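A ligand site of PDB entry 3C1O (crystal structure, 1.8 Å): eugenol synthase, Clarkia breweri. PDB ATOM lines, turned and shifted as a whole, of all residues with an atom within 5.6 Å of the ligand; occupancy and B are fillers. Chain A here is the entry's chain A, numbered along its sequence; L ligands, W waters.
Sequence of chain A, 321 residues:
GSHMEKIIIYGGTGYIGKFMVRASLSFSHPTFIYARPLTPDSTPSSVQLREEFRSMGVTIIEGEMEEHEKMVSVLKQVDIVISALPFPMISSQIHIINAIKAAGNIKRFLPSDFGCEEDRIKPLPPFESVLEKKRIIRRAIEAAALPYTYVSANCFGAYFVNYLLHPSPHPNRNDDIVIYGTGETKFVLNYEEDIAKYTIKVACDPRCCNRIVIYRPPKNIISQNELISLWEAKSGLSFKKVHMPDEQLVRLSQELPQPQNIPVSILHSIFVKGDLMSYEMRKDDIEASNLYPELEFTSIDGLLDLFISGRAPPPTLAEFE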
ATOM      1  N   GLY A  11      23.149 -12.944 -17.551  1.00  0.00           N
ATOM      2  CA  GLY A  11      22.358 -12.108 -16.664  1.00  0.00           C
ATOM      3  C   GLY A  11      23.142 -10.844 -16.354  1.00  0.00           C
ATOM      4  O   GLY A  11      22.946 -10.218 -15.311  1.00  0.00           O
ATOM      5  N   GLY A  12      24.023 -10.475 -17.276  1.00  0.00           N
ATOM      6  CA  GLY A  12      24.868  -9.306 -17.093  1.00  0.00           C
ATOM      7  C   GLY A  12      24.152  -7.972 -17.028  1.00  0.00           C
ATOM      8  O   GLY A  12      24.723  -6.984 -16.548  1.00  0.00           O
ATOM      9  N   THR A  13      22.918  -7.906 -17.515  1.00  0.00           N
ATOM     10  CA  THR A  13      22.156  -6.665 -17.487  1.00  0.00           C
ATOM     11  C   THR A  13      21.224  -6.642 -16.279  1.00  0.00           C
ATOM     12  O   THR A  13      20.366  -5.760 -16.162  1.00  0.00           O
ATOM     13  CB  THR A  13      21.337  -6.493 -18.775  1.00  0.00           C
ATOM     14  OG1 THR A  13      20.583  -7.677 -19.026  1.00  0.00           O
ATOM     15  CG2 THR A  13      22.263  -6.221 -19.964  1.00  0.00           C
ATOM     16  N   GLY A  14      21.396  -7.627 -15.399  1.00  0.00           N
ATOM     17  CA  GLY A  14      20.577  -7.721 -14.199  1.00  0.00           C
ATOM     18  C   GLY A  14      21.014  -6.800 -13.066  1.00  0.00           C
ATOM     19  O   GLY A  14      22.013  -6.079 -13.174  1.00  0.00           O
ATOM     20  N   TYR A  15      20.273  -6.844 -11.959  1.00  0.00           N
ATOM     21  CA  TYR A  15      20.567  -5.991 -10.819  1.00  0.00           C
ATOM     22  C   TYR A  15      22.002  -6.160 -10.309  1.00  0.00           C
ATOM     23  O   TYR A  15      22.747  -5.180 -10.224  1.00  0.00           O
ATOM     24  CB  TYR A  15      19.581  -6.278  -9.670  1.00  0.00           C
ATOM     25  CG  TYR A  15      19.857  -5.433  -8.451  1.00  0.00           C
ATOM     26  CD1 TYR A  15      19.512  -4.074  -8.436  1.00  0.00           C
ATOM     27  CD2 TYR A  15      20.502  -5.965  -7.341  1.00  0.00           C
ATOM     28  CE1 TYR A  15      19.816  -3.277  -7.340  1.00  0.00           C
ATOM     29  CE2 TYR A  15      20.800  -5.172  -6.237  1.00  0.00           C
ATOM     30  CZ  TYR A  15      20.456  -3.825  -6.243  1.00  0.00           C
ATOM     31  OH  TYR A  15      20.753  -3.035  -5.156  1.00  0.00           O
ATOM     32  N   ILE A  16      22.399  -7.384  -9.977  1.00  0.00           N
ATOM     33  CA  ILE A  16      23.762  -7.604  -9.511  1.00  0.00           C
ATOM     34  C   ILE A  16      24.667  -7.851 -10.715  1.00  0.00           C
ATOM     35  O   ILE A  16      25.862  -7.556 -10.678  1.00  0.00           O
ATOM     36  CB  ILE A  16      23.874  -8.804  -8.520  1.00  0.00           C
ATOM     37  CG1 ILE A  16      25.198  -8.722  -7.761  1.00  0.00           C
ATOM     38  CG2 ILE A  16      23.789 -10.123  -9.266  1.00  0.00           C
ATOM     39  CD1 ILE A  16      25.290  -7.543  -6.794  1.00  0.00           C
ATOM     40  N   GLY A  17      24.081  -8.367 -11.792  1.00  0.00           N
ATOM     41  CA  GLY A  17      24.847  -8.646 -12.992  1.00  0.00           C
ATOM     42  C   GLY A  17      25.579  -7.434 -13.547  1.00  0.00           C
ATOM     43  O   GLY A  17      26.730  -7.537 -13.966  1.00  0.00           O
ATOM     44  N   ARG A  36      19.821 -12.331 -23.975  1.00  0.00           N
ATOM     45  CA  ARG A  36      18.711 -12.675 -24.846  1.00  0.00           C
ATOM     46  C   ARG A  36      18.500 -11.538 -25.824  1.00  0.00           C
ATOM     47  O   ARG A  36      18.779 -10.372 -25.510  1.00  0.00           O
ATOM     48  CB  ARG A  36      17.425 -12.917 -24.037  1.00  0.00           C
ATOM     49  CG  ARG A  36      16.925 -11.696 -23.276  1.00  0.00           C
ATOM     50  CD  ARG A  36      15.572 -11.986 -22.630  1.00  0.00           C
ATOM     51  NE  ARG A  36      15.245 -10.996 -21.601  1.00  0.00           N
ATOM     52  CZ  ARG A  36      14.167 -11.073 -20.828  1.00  0.00           C
ATOM     53  NH1 ARG A  36      13.321 -12.084 -20.964  1.00  0.00           N
ATOM     54  NH2 ARG A  36      13.947 -10.146 -19.901  1.00  0.00           N
ATOM     55  N   LEU A  38      16.821  -8.581 -27.912  1.00  0.00           N
ATOM     56  CA  LEU A  38      15.867  -7.579 -27.482  1.00  0.00           C
ATOM     57  C   LEU A  38      14.531  -7.780 -28.187  1.00  0.00           C
ATOM     58  O   LEU A  38      14.468  -8.305 -29.295  1.00  0.00           O
ATOM     59  CB  LEU A  38      16.392  -6.173 -27.782  1.00  0.00           C
ATOM     60  CG  LEU A  38      17.468  -5.621 -26.842  1.00  0.00           C
ATOM     61  CD1 LEU A  38      17.986  -4.290 -27.363  1.00  0.00           C
ATOM     62  CD2 LEU A  38      16.874  -5.447 -25.446  1.00  0.00           C
ATOM     63  N   THR A  43      12.398  -3.670 -21.615  1.00  0.00           N
ATOM     64  CA  THR A  43      12.373  -2.460 -20.810  1.00  0.00           C
ATOM     65  C   THR A  43      13.446  -1.501 -21.323  1.00  0.00           C
ATOM     66  O   THR A  43      14.548  -1.925 -21.664  1.00  0.00           O
ATOM     67  CB  THR A  43      12.659  -2.778 -19.319  1.00  0.00           C
ATOM     68  OG1 THR A  43      13.987  -3.289 -19.176  1.00  0.00           O
ATOM     69  CG2 THR A  43      11.666  -3.806 -18.792  1.00  0.00           C
ATOM     70  N   SER A  46      16.852  -2.105 -19.990  1.00  0.00           N
ATOM     71  CA  SER A  46      17.638  -3.196 -20.544  1.00  0.00           C
ATOM     72  C   SER A  46      18.290  -2.764 -21.856  1.00  0.00           C
ATOM     73  O   SER A  46      19.417  -3.157 -22.158  1.00  0.00           O
ATOM     74  CB  SER A  46      16.745  -4.416 -20.807  1.00  0.00           C
ATOM     75  OG  SER A  46      15.855  -4.180 -21.884  1.00  0.00           O
ATOM     76  N   ARG A  50      22.589  -2.313 -22.468  1.00  0.00           N
ATOM     77  CA  ARG A  50      23.315  -2.971 -23.538  1.00  0.00           C
ATOM     78  C   ARG A  50      24.117  -1.940 -24.340  1.00  0.00           C
ATOM     79  O   ARG A  50      25.255  -2.197 -24.728  1.00  0.00           O
ATOM     80  CB  ARG A  50      22.339  -3.715 -24.460  1.00  0.00           C
ATOM     81  CG  ARG A  50      21.718  -4.978 -23.844  1.00  0.00           C
ATOM     82  CD  ARG A  50      20.598  -5.490 -24.747  1.00  0.00           C
ATOM     83  NE  ARG A  50      20.126  -6.850 -24.448  1.00  0.00           N
ATOM     84  CZ  ARG A  50      19.485  -7.201 -23.342  1.00  0.00           C
ATOM     85  NH1 ARG A  50      19.227  -6.313 -22.398  1.00  0.00           N
ATOM     86  NH2 ARG A  50      19.077  -8.460 -23.197  1.00  0.00           N
ATOM     87  N   MET A  65      19.247 -19.544 -24.508  1.00  0.00           N
ATOM     88  CA  MET A  65      19.996 -20.531 -23.741  1.00  0.00           C
ATOM     89  C   MET A  65      20.065 -21.881 -24.451  1.00  0.00           C
ATOM     90  O   MET A  65      21.014 -22.650 -24.248  1.00  0.00           O
ATOM     91  CB  MET A  65      19.352 -20.721 -22.365  1.00  0.00           C
ATOM     92  CG  MET A  65      19.354 -19.472 -21.487  1.00  0.00           C
ATOM     93  SD  MET A  65      21.035 -18.922 -21.088  1.00  0.00           S
ATOM     94  CE  MET A  65      21.426 -20.002 -19.734  1.00  0.00           C
ATOM     95  N   ALA A  84      24.574 -14.614 -13.270  1.00  0.00           N
ATOM     96  CA  ALA A  84      23.843 -13.763 -12.343  1.00  0.00           C
ATOM     97  C   ALA A  84      22.363 -13.763 -12.758  1.00  0.00           C
ATOM     98  O   ALA A  84      21.657 -12.768 -12.598  1.00  0.00           O
ATOM     99  CB  ALA A  84      24.401 -12.335 -12.396  1.00  0.00           C
ATOM    100  N   LEU A  85      21.906 -14.894 -13.289  1.00  0.00           N
ATOM    101  CA  LEU A  85      20.526 -15.029 -13.733  1.00  0.00           C
ATOM    102  C   LEU A  85      19.551 -15.076 -12.560  1.00  0.00           C
ATOM    103  O   LEU A  85      19.887 -15.523 -11.478  1.00  0.00           O
ATOM    104  CB  LEU A  85      20.369 -16.292 -14.579  1.00  0.00           C
ATOM    105  CG  LEU A  85      21.079 -16.248 -15.931  1.00  0.00           C
ATOM    106  CD1 LEU A  85      21.119 -17.656 -16.534  1.00  0.00           C
ATOM    107  CD2 LEU A  85      20.357 -15.270 -16.852  1.00  0.00           C
ATOM    108  N   PRO A  86      18.303 -14.592 -12.774  1.00  0.00           N
ATOM    109  CA  PRO A  86      17.289 -14.580 -11.716  1.00  0.00           C
ATOM    110  C   PRO A  86      16.657 -15.949 -11.469  1.00  0.00           C
ATOM    111  O   PRO A  86      16.837 -16.882 -12.262  1.00  0.00           O
ATOM    112  CB  PRO A  86      16.288 -13.549 -12.220  1.00  0.00           C
ATOM    113  CG  PRO A  86      16.337 -13.742 -13.701  1.00  0.00           C
ATOM    114  CD  PRO A  86      17.829 -13.890 -13.972  1.00  0.00           C
ATOM    115  N   PHE A  87      15.928 -16.065 -10.372  1.00  0.00           N
ATOM    116  CA  PHE A  87      15.284 -17.329  -9.997  1.00  0.00           C
ATOM    117  C   PHE A  87      14.535 -18.071 -11.100  1.00  0.00           C
ATOM    118  O   PHE A  87      14.649 -19.302 -11.200  1.00  0.00           O
ATOM    119  CB  PHE A  87      14.366 -17.117  -8.796  1.00  0.00           C
ATOM    120  CG  PHE A  87      15.022 -17.438  -7.485  1.00  0.00           C
ATOM    121  CD1 PHE A  87      15.315 -18.771  -7.160  1.00  0.00           C
ATOM    122  CD2 PHE A  87      15.375 -16.436  -6.597  1.00  0.00           C
ATOM    123  CE1 PHE A  87      15.948 -19.088  -5.960  1.00  0.00           C
ATOM    124  CE2 PHE A  87      16.020 -16.741  -5.395  1.00  0.00           C
ATOM    125  CZ  PHE A  87      16.305 -18.073  -5.075  1.00  0.00           C
ATOM    126  N   MET A  89      15.205 -18.235 -14.078  1.00  0.00           N
ATOM    127  CA  MET A  89      16.177 -18.726 -15.058  1.00  0.00           C
ATOM    128  C   MET A  89      17.217 -19.662 -14.452  1.00  0.00           C
ATOM    129  O   MET A  89      18.141 -20.088 -15.145  1.00  0.00           O
ATOM    130  CB  MET A  89      16.895 -17.542 -15.724  1.00  0.00           C
ATOM    131  CG  MET A  89      16.024 -16.736 -16.682  1.00  0.00           C
ATOM    132  SD  MET A  89      15.443 -17.754 -18.052  1.00  0.00           S
ATOM    133  CE  MET A  89      16.951 -17.926 -19.009  1.00  0.00           C
ATOM    134  N   ILE A  90      17.089 -19.968 -13.168  1.00  0.00           N
ATOM    135  CA  ILE A  90      18.051 -20.848 -12.526  1.00  0.00           C
ATOM    136  C   ILE A  90      18.192 -22.200 -13.200  1.00  0.00           C
ATOM    137  O   ILE A  90      19.298 -22.627 -13.512  1.00  0.00           O
ATOM    138  CB  ILE A  90      17.700 -21.055 -11.033  1.00  0.00           C
ATOM    139  CG1 ILE A  90      17.842 -19.726 -10.281  1.00  0.00           C
ATOM    140  CG2 ILE A  90      18.619 -22.106 -10.408  1.00  0.00           C
ATOM    141  CD1 ILE A  90      19.191 -19.045 -10.454  1.00  0.00           C
ATOM    142  N   SER A 112      24.582 -18.950 -10.466  1.00  0.00           N
ATOM    143  CA  SER A 112      23.872 -17.870  -9.809  1.00  0.00           C
ATOM    144  C   SER A 112      23.397 -18.261  -8.412  1.00  0.00           C
ATOM    145  O   SER A 112      22.247 -18.667  -8.225  1.00  0.00           O
ATOM    146  CB  SER A 112      22.678 -17.424 -10.662  1.00  0.00           C
ATOM    147  OG  SER A 112      22.151 -16.195 -10.207  1.00  0.00           O
ATOM    148  N   ASP A 113      24.303 -18.171  -7.435  1.00  0.00           N
ATOM    149  CA  ASP A 113      23.985 -18.459  -6.041  1.00  0.00           C
ATOM    150  C   ASP A 113      23.842 -17.075  -5.432  1.00  0.00           C
ATOM    151  O   ASP A 113      22.742 -16.528  -5.386  1.00  0.00           O
ATOM    152  CB  ASP A 113      25.139 -19.227  -5.382  1.00  0.00           C
ATOM    153  CG  ASP A 113      25.041 -20.725  -5.585  1.00  0.00           C
ATOM    154  OD1 ASP A 113      24.035 -21.183  -6.176  1.00  0.00           O
ATOM    155  OD2 ASP A 113      25.964 -21.454  -5.152  1.00  0.00           O
ATOM    156  N   PHE A 114      24.959 -16.513  -4.958  1.00  0.00           N
ATOM    157  CA  PHE A 114      24.982 -15.167  -4.407  1.00  0.00           C
ATOM    158  C   PHE A 114      23.945 -14.858  -3.340  1.00  0.00           C
ATOM    159  O   PHE A 114      23.406 -13.760  -3.272  1.00  0.00           O
ATOM    160  CB  PHE A 114      24.870 -14.150  -5.557  1.00  0.00           C
ATOM    161  CG  PHE A 114      25.959 -14.286  -6.584  1.00  0.00           C
ATOM    162  CD1 PHE A 114      27.279 -13.991  -6.262  1.00  0.00           C
ATOM    163  CD2 PHE A 114      25.682 -14.777  -7.854  1.00  0.00           C
ATOM    164  CE1 PHE A 114      28.307 -14.179  -7.186  1.00  0.00           C
ATOM    165  CE2 PHE A 114      26.695 -14.972  -8.794  1.00  0.00           C
ATOM    166  CZ  PHE A 114      28.016 -14.674  -8.454  1.00  0.00           C
ATOM    167  N   GLY A 115      23.667 -15.835  -2.487  1.00  0.00           N
ATOM    168  CA  GLY A 115      22.698 -15.592  -1.443  1.00  0.00           C
ATOM    169  C   GLY A 115      23.262 -16.160  -0.177  1.00  0.00           C
ATOM    170  O   GLY A 115      24.355 -15.791   0.266  1.00  0.00           O
ATOM    171  N   CYS A 116      22.489 -17.083   0.395  1.00  0.00           N
ATOM    172  CA  CYS A 116      22.845 -17.805   1.606  1.00  0.00           C
ATOM    173  C   CYS A 116      23.644 -19.018   1.122  1.00  0.00           C
ATOM    174  O   CYS A 116      23.913 -19.150  -0.064  1.00  0.00           O
ATOM    175  CB  CYS A 116      21.571 -18.286   2.283  1.00  0.00           C
ATOM    176  SG  CYS A 116      20.465 -19.192   1.149  1.00  0.00           S
ATOM    177  N   LYS A 134      18.552 -24.265  -7.171  1.00  0.00           N
ATOM    178  CA  LYS A 134      19.970 -23.933  -7.158  1.00  0.00           C
ATOM    179  C   LYS A 134      20.810 -25.157  -6.770  1.00  0.00           C
ATOM    180  O   LYS A 134      21.913 -25.342  -7.276  1.00  0.00           O
ATOM    181  CB  LYS A 134      20.251 -22.756  -6.222  1.00  0.00           C
ATOM    182  CG  LYS A 134      19.685 -21.433  -6.737  1.00  0.00           C
ATOM    183  CD  LYS A 134      20.129 -20.238  -5.882  1.00  0.00           C
ATOM    184  CE  LYS A 134      19.690 -18.931  -6.539  1.00  0.00           C
ATOM    185  NZ  LYS A 134      20.017 -17.708  -5.722  1.00  0.00           N
ATOM    186  N   ALA A 153      27.003 -14.575  -0.962  1.00  0.00           N
ATOM    187  CA  ALA A 153      27.263 -13.144  -0.852  1.00  0.00           C
ATOM    188  C   ALA A 153      26.574 -12.506   0.343  1.00  0.00           C
ATOM    189  O   ALA A 153      26.900 -11.375   0.724  1.00  0.00           O
ATOM    190  CB  ALA A 153      26.832 -12.448  -2.135  1.00  0.00           C
ATOM    191  N   ASN A 154      25.631 -13.235   0.931  1.00  0.00           N
ATOM    192  CA  ASN A 154      24.832 -12.723   2.035  1.00  0.00           C
ATOM    193  C   ASN A 154      23.973 -11.578   1.499  1.00  0.00           C
ATOM    194  O   ASN A 154      23.817 -11.439   0.293  1.00  0.00           O
ATOM    195  CB  ASN A 154      25.716 -12.323   3.225  1.00  0.00           C
ATOM    196  CG  ASN A 154      26.114 -13.527   4.072  1.00  0.00           C
ATOM    197  OD1 ASN A 154      25.282 -14.391   4.360  1.00  0.00           O
ATOM    198  ND2 ASN A 154      27.379 -13.592   4.456  1.00  0.00           N
ATOM    199  N   CYS A 155      23.404 -10.747   2.377  1.00  0.00           N
ATOM    200  CA  CYS A 155      22.511  -9.690   1.913  1.00  0.00           C
ATOM    201  C   CYS A 155      23.074  -8.580   1.031  1.00  0.00           C
ATOM    202  O   CYS A 155      24.034  -7.916   1.415  1.00  0.00           O
ATOM    203  CB  CYS A 155      21.812  -9.042   3.107  1.00  0.00           C
ATOM    204  SG  CYS A 155      20.801 -10.182   4.064  1.00  0.00           S
ATOM    205  N   PHE A 156      22.463  -8.380  -0.130  1.00  0.00           N
ATOM    206  CA  PHE A 156      22.849  -7.303  -1.022  1.00  0.00           C
ATOM    207  C   PHE A 156      22.554  -6.026  -0.216  1.00  0.00           C
ATOM    208  O   PHE A 156      21.403  -5.766   0.137  1.00  0.00           O
ATOM    209  CB  PHE A 156      22.022  -7.314  -2.309  1.00  0.00           C
ATOM    210  CG  PHE A 156      22.426  -8.374  -3.301  1.00  0.00           C
ATOM    211  CD1 PHE A 156      23.418  -9.302  -2.988  1.00  0.00           C
ATOM    212  CD2 PHE A 156      21.807  -8.450  -4.549  1.00  0.00           C
ATOM    213  CE1 PHE A 156      23.784 -10.301  -3.912  1.00  0.00           C
ATOM    214  CE2 PHE A 156      22.171  -9.441  -5.469  1.00  0.00           C
ATOM    215  CZ  PHE A 156      23.156 -10.364  -5.144  1.00  0.00           C
ATOM    216  N   TYR A 159      20.167  -3.138  -1.691  1.00  0.00           N
ATOM    217  CA  TYR A 159      18.919  -3.849  -1.896  1.00  0.00           C
ATOM    218  C   TYR A 159      18.140  -3.950  -0.575  1.00  0.00           C
ATOM    219  O   TYR A 159      16.988  -3.546  -0.491  1.00  0.00           O
ATOM    220  CB  TYR A 159      19.229  -5.243  -2.433  1.00  0.00           C
ATOM    221  CG  TYR A 159      18.031  -6.111  -2.759  1.00  0.00           C
ATOM    222  CD1 TYR A 159      17.493  -6.127  -4.049  1.00  0.00           C
ATOM    223  CD2 TYR A 159      17.468  -6.943  -1.796  1.00  0.00           C
ATOM    224  CE1 TYR A 159      16.423  -6.972  -4.366  1.00  0.00           C
ATOM    225  CE2 TYR A 159      16.406  -7.790  -2.107  1.00  0.00           C
ATOM    226  CZ  TYR A 159      15.888  -7.794  -3.389  1.00  0.00           C
ATOM    227  OH  TYR A 159      14.838  -8.627  -3.697  1.00  0.00           O
ATOM    228  N   PHE A 160      18.799  -4.464   0.461  1.00  0.00           N
ATOM    229  CA  PHE A 160      18.133  -4.615   1.748  1.00  0.00           C
ATOM    230  C   PHE A 160      17.938  -3.326   2.551  1.00  0.00           C
ATOM    231  O   PHE A 160      16.992  -3.233   3.334  1.00  0.00           O
ATOM    232  CB  PHE A 160      18.840  -5.693   2.566  1.00  0.00           C
ATOM    233  CG  PHE A 160      18.297  -7.078   2.309  1.00  0.00           C
ATOM    234  CD1 PHE A 160      17.110  -7.487   2.900  1.00  0.00           C
ATOM    235  CD2 PHE A 160      18.919  -7.929   1.402  1.00  0.00           C
ATOM    236  CE1 PHE A 160      16.538  -8.714   2.585  1.00  0.00           C
ATOM    237  CE2 PHE A 160      18.362  -9.161   1.081  1.00  0.00           C
ATOM    238  CZ  PHE A 160      17.166  -9.560   1.671  1.00  0.00           C
ATOM    239  N   LEU A 317      12.747  -4.066  -7.665  1.00  0.00           N
ATOM    240  CA  LEU A 317      11.853  -5.179  -7.359  1.00  0.00           C
ATOM    241  C   LEU A 317      12.618  -6.381  -6.817  1.00  0.00           C
ATOM    242  O   LEU A 317      13.301  -7.016  -7.652  1.00  0.00           O
ATOM    243  CB  LEU A 317      11.077  -5.577  -8.622  1.00  0.00           C
ATOM    244  CG  LEU A 317      10.111  -4.508  -9.117  1.00  0.00           C
ATOM    245  CD1 LEU A 317       9.529  -4.898 -10.473  1.00  0.00           C
ATOM    246  CD2 LEU A 317       9.001  -4.322  -8.087  1.00  0.00           C
HETATM  247  P1  LIG L   1      17.601  -9.820 -12.080  1.00  0.00           P
HETATM  248  O1  LIG L   1      16.160 -10.165 -12.006  1.00  0.00           O
HETATM  249  O2  LIG L   1      18.049  -8.415 -11.949  1.00  0.00           O
HETATM  250  O3  LIG L   1      18.137 -10.502 -13.414  1.00  0.00           O
HETATM  251  C1  LIG L   1      17.452 -10.337 -14.651  1.00  0.00           C
HETATM  252  C2  LIG L   1      18.517 -10.551 -15.691  1.00  0.00           C
HETATM  253  O4  LIG L   1      18.506 -11.818 -16.559  1.00  0.00           O
HETATM  254  C3  LIG L   1      18.578  -9.555 -16.815  1.00  0.00           C
HETATM  255  O5  LIG L   1      19.947  -9.465 -17.187  1.00  0.00           O
HETATM  256  C4  LIG L   1      17.759 -10.100 -17.981  1.00  0.00           C
HETATM  257  O6  LIG L   1      18.101  -9.629 -19.253  1.00  0.00           O
HETATM  258  C5  LIG L   1      17.861 -11.591 -17.811  1.00  0.00           C
HETATM  259  N1  LIG L   1      16.601 -12.325 -17.929  1.00  0.00           N
HETATM  260  C6  LIG L   1      15.454 -12.209 -17.165  1.00  0.00           C
HETATM  261  N2  LIG L   1      14.503 -13.039 -17.552  1.00  0.00           N
HETATM  262  C7  LIG L   1      15.049 -13.709 -18.607  1.00  0.00           C
HETATM  263  C8  LIG L   1      14.552 -14.735 -19.462  1.00  0.00           C
HETATM  264  N3  LIG L   1      13.316 -15.228 -19.322  1.00  0.00           N
HETATM  265  N4  LIG L   1      15.390 -15.203 -20.453  1.00  0.00           N
HETATM  266  C9  LIG L   1      16.647 -14.708 -20.590  1.00  0.00           C
HETATM  267  N5  LIG L   1      17.222 -13.735 -19.824  1.00  0.00           N
HETATM  268  C10 LIG L   1      16.352 -13.291 -18.844  1.00  0.00           C
HETATM  269  O7  LIG L   1      18.378 -10.821 -11.064  1.00  0.00           O
HETATM  270  P2  LIG L   1      19.005 -10.410  -9.663  1.00  0.00           P
HETATM  271  O8  LIG L   1      18.003  -9.738  -8.811  1.00  0.00           O
HETATM  272  O9  LIG L   1      20.253  -9.646  -9.981  1.00  0.00           O
HETATM  273  O10 LIG L   1      19.435 -11.799  -9.025  1.00  0.00           O
HETATM  274  C11 LIG L   1      20.540 -12.581  -9.539  1.00  0.00           C
HETATM  275  C12 LIG L   1      21.031 -13.536  -8.464  1.00  0.00           C
HETATM  276  O11 LIG L   1      21.273 -12.760  -7.258  1.00  0.00           O
HETATM  277  C13 LIG L   1      20.036 -14.680  -8.139  1.00  0.00           C
HETATM  278  O12 LIG L   1      20.698 -15.907  -7.938  1.00  0.00           O
HETATM  279  C14 LIG L   1      19.366 -14.122  -6.912  1.00  0.00           C
HETATM  280  O13 LIG L   1      18.823 -15.171  -6.143  1.00  0.00           O
HETATM  281  C15 LIG L   1      20.445 -13.347  -6.216  1.00  0.00           C
HETATM  282  N6  LIG L   1      19.893 -12.336  -5.281  1.00  0.00           N
HETATM  283  C16 LIG L   1      20.463 -12.289  -4.017  1.00  0.00           C
HETATM  284  C17 LIG L   1      20.114 -11.266  -3.134  1.00  0.00           C
HETATM  285  C18 LIG L   1      20.768 -11.132  -1.782  1.00  0.00           C
HETATM  286  O14 LIG L   1      20.407 -10.248  -1.012  1.00  0.00           O
HETATM  287  N7  LIG L   1      21.755 -11.995  -1.487  1.00  0.00           N
HETATM  288  C19 LIG L   1      19.108 -10.320  -3.515  1.00  0.00           C
HETATM  289  C20 LIG L   1      18.547 -10.379  -4.794  1.00  0.00           C
HETATM  290  C21 LIG L   1      18.953 -11.374  -5.687  1.00  0.00           C
HETATM  291  P3  LIG L   1      17.316  -8.393 -19.942  1.00  0.00           P
HETATM  292  O15 LIG L   1      18.176  -7.160 -19.791  1.00  0.00           O
HETATM  293  O16 LIG L   1      17.133  -8.913 -21.343  1.00  0.00           O
HETATM  294  O17 LIG L   1      16.001  -8.239 -19.191  1.00  0.00           O
HETATM  295  O   HOH W   1      16.710  -6.243 -13.309  1.00  0.00           O
HETATM  296  O   HOH W   2      21.721  -9.889 -12.266  1.00  0.00           O
HETATM  297  O   HOH W   3      19.757 -11.969 -20.974  1.00  0.00           O
HETATM  298  O   HOH W   4      15.178  -7.757 -22.844  1.00  0.00           O
HETATM  299  O   HOH W   5      18.071  -5.347 -17.429  1.00  0.00           O
HETATM  300  O   HOH W   6      14.172 -10.763 -13.759  1.00  0.00           O
HETATM  301  O   HOH W   7      15.134 -11.150  -9.569  1.00  0.00           O
HETATM  302  O   HOH W   8      16.193 -13.601  -5.846  1.00  0.00           O
HETATM  303  O   HOH W   9      21.364  -9.889 -20.489  1.00  0.00           O
HETATM  304  O   HOH W  10      16.304  -7.287  -8.400  1.00  0.00           O
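O of Ser 112 sits close to NZ of Lys 134, at 3.5 Å.
N of Asn 154 sits at hydrogen-bond distance from O of Gly 115 (2.9 Å).
O of Leu 85 is in hydrogen-bond range of OG of Ser 112 (2.7 Å).
The side-chain hydroxyl of Ser 46 lies within hydrogen-bond range of the backbone carbonyl oxygen of Thr 43 (2.6 Å).
The guanidinium group (NH2) of Arg 50 lies within hydrogen-bond range of the backbone carbonyl oxygen (O) of Arg 36.
The side-chain amino group of Lys 134 lies within hydrogen-bond range of the backbone carbonyl oxygen of Asp 113, at 3.0 Å.
NH1 of Arg 50 lies within hydrogen-bond range of O of Ser 46 (3.2 Å).
The backbone carbonyl oxygen of Gly 115 sits at hydrogen-bond distance from the backbone NH of Ala 153 (3.2 Å).
Gly 11 touches the ligand (C to O5, 3.6 Å).
Ser 46 touches the ligand.
Ala 84 touches the ligand (O to C11, 3.3 Å).
Leu 85 touches the ligand.
Pro 86 touches the ligand.
Phe 87 touches the ligand (CE2 to O13, 3.3 Å).
Gly 115 touches the ligand.
Cys 155 touches the ligand (CA to O14, 3.6 Å).
Tyr 159 touches the ligand (CE2 to C19, 3.96 Å).
CE2 of Phe 160 touches O14 of the ligand (3.1 Å).
Hydrophobic or aromatic side chains that line the ligand: Tyr 15, Ile 16, Leu 85, Pro 86, Phe 87, Met 89, Phe 156, Tyr 159 and Phe 160.
Within 4 Å of the ligand: Gly 11, Thr 13, Gly 14, Tyr 15, Ile 16, Arg 36, Ser 46, Arg 50, Ala 84, Leu 85, Pro 86, Phe 87, Met 89, Ser 112, Asp 113, Phe 114, Gly 115, Lys 134, Asn 154, Cys 155, Phe 156, Tyr 159 and Phe 160.
The nearest printed residue that does not touch the ligand is Gly 12 (4.2 Å).
O of Asp 113 is in hydrogen-bond range of O12 of the ligand (3.3 Å).
The side-chain hydroxyl of Ser 112 is in hydrogen-bond range of an oxygen (O12) of the ligand (2.7 Å).
O16 of the ligand lies within salt-bridge range of NE of Arg 36 (2.8 Å).
N3 of the ligand lies close to SD of Met 89 (3.5 Å).
O16 of the ligand lies within salt-bridge range of NH2 of Arg 50.
O of Phe 114 is in hydrogen-bond range of N7 of the ligand, 3.0 Å away.
The backbone NH (N) of Tyr 15 is in hydrogen-bond range of an oxygen (O2) of the ligand (2.7 Å).
N of Gly 14 sits at hydrogen-bond distance from O5 of the ligand.
N of Thr 13 lies close to O5 of the ligand (3.4 Å).
The backbone carbonyl oxygen (O) of Asn 154 is in hydrogen-bond range of a nitrogen (N7) of the ligand (2.8 Å).
O12 of the ligand sits at hydrogen-bond distance from O of Ser 112 (3.2 Å).
N of Phe 156 sits at hydrogen-bond distance from O14 of the ligand (2.9 Å).
The side-chain amino group (NZ) of Lys 134 is in hydrogen-bond range of an oxygen (O13) of the ligand (2.8 Å).
The side-chain hydroxyl (OG1) of Thr 13 sits at hydrogen-bond distance from an oxygen (O15) of the ligand, 2.6 Å away.
An oxygen (O9) of the ligand sits at hydrogen-bond distance from the backbone NH (N) of Ile 16 (3.1 Å).
Water W4 bridges O16 of the ligand (2.7 Å) and NE of Arg 36 (3.5 Å).
Water W5 bridges the backbone carbonyl oxygen (O) of Thr 13 (2.7 Å) and an oxygen (O15) of the ligand (3.0 Å).
Water W10 lies within hydrogen-bond range of O8 of the ligand (3.0 Å) and O of Leu 317 (3.1 Å).
Water W3 bridges N of Arg 36 and N5 of the ligand.
Water W9 lies within hydrogen-bond range of the side-chain hydroxyl (OG1) of Thr 13 (2.8 Å) and an oxygen (O6) of the ligand (3.5 Å).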
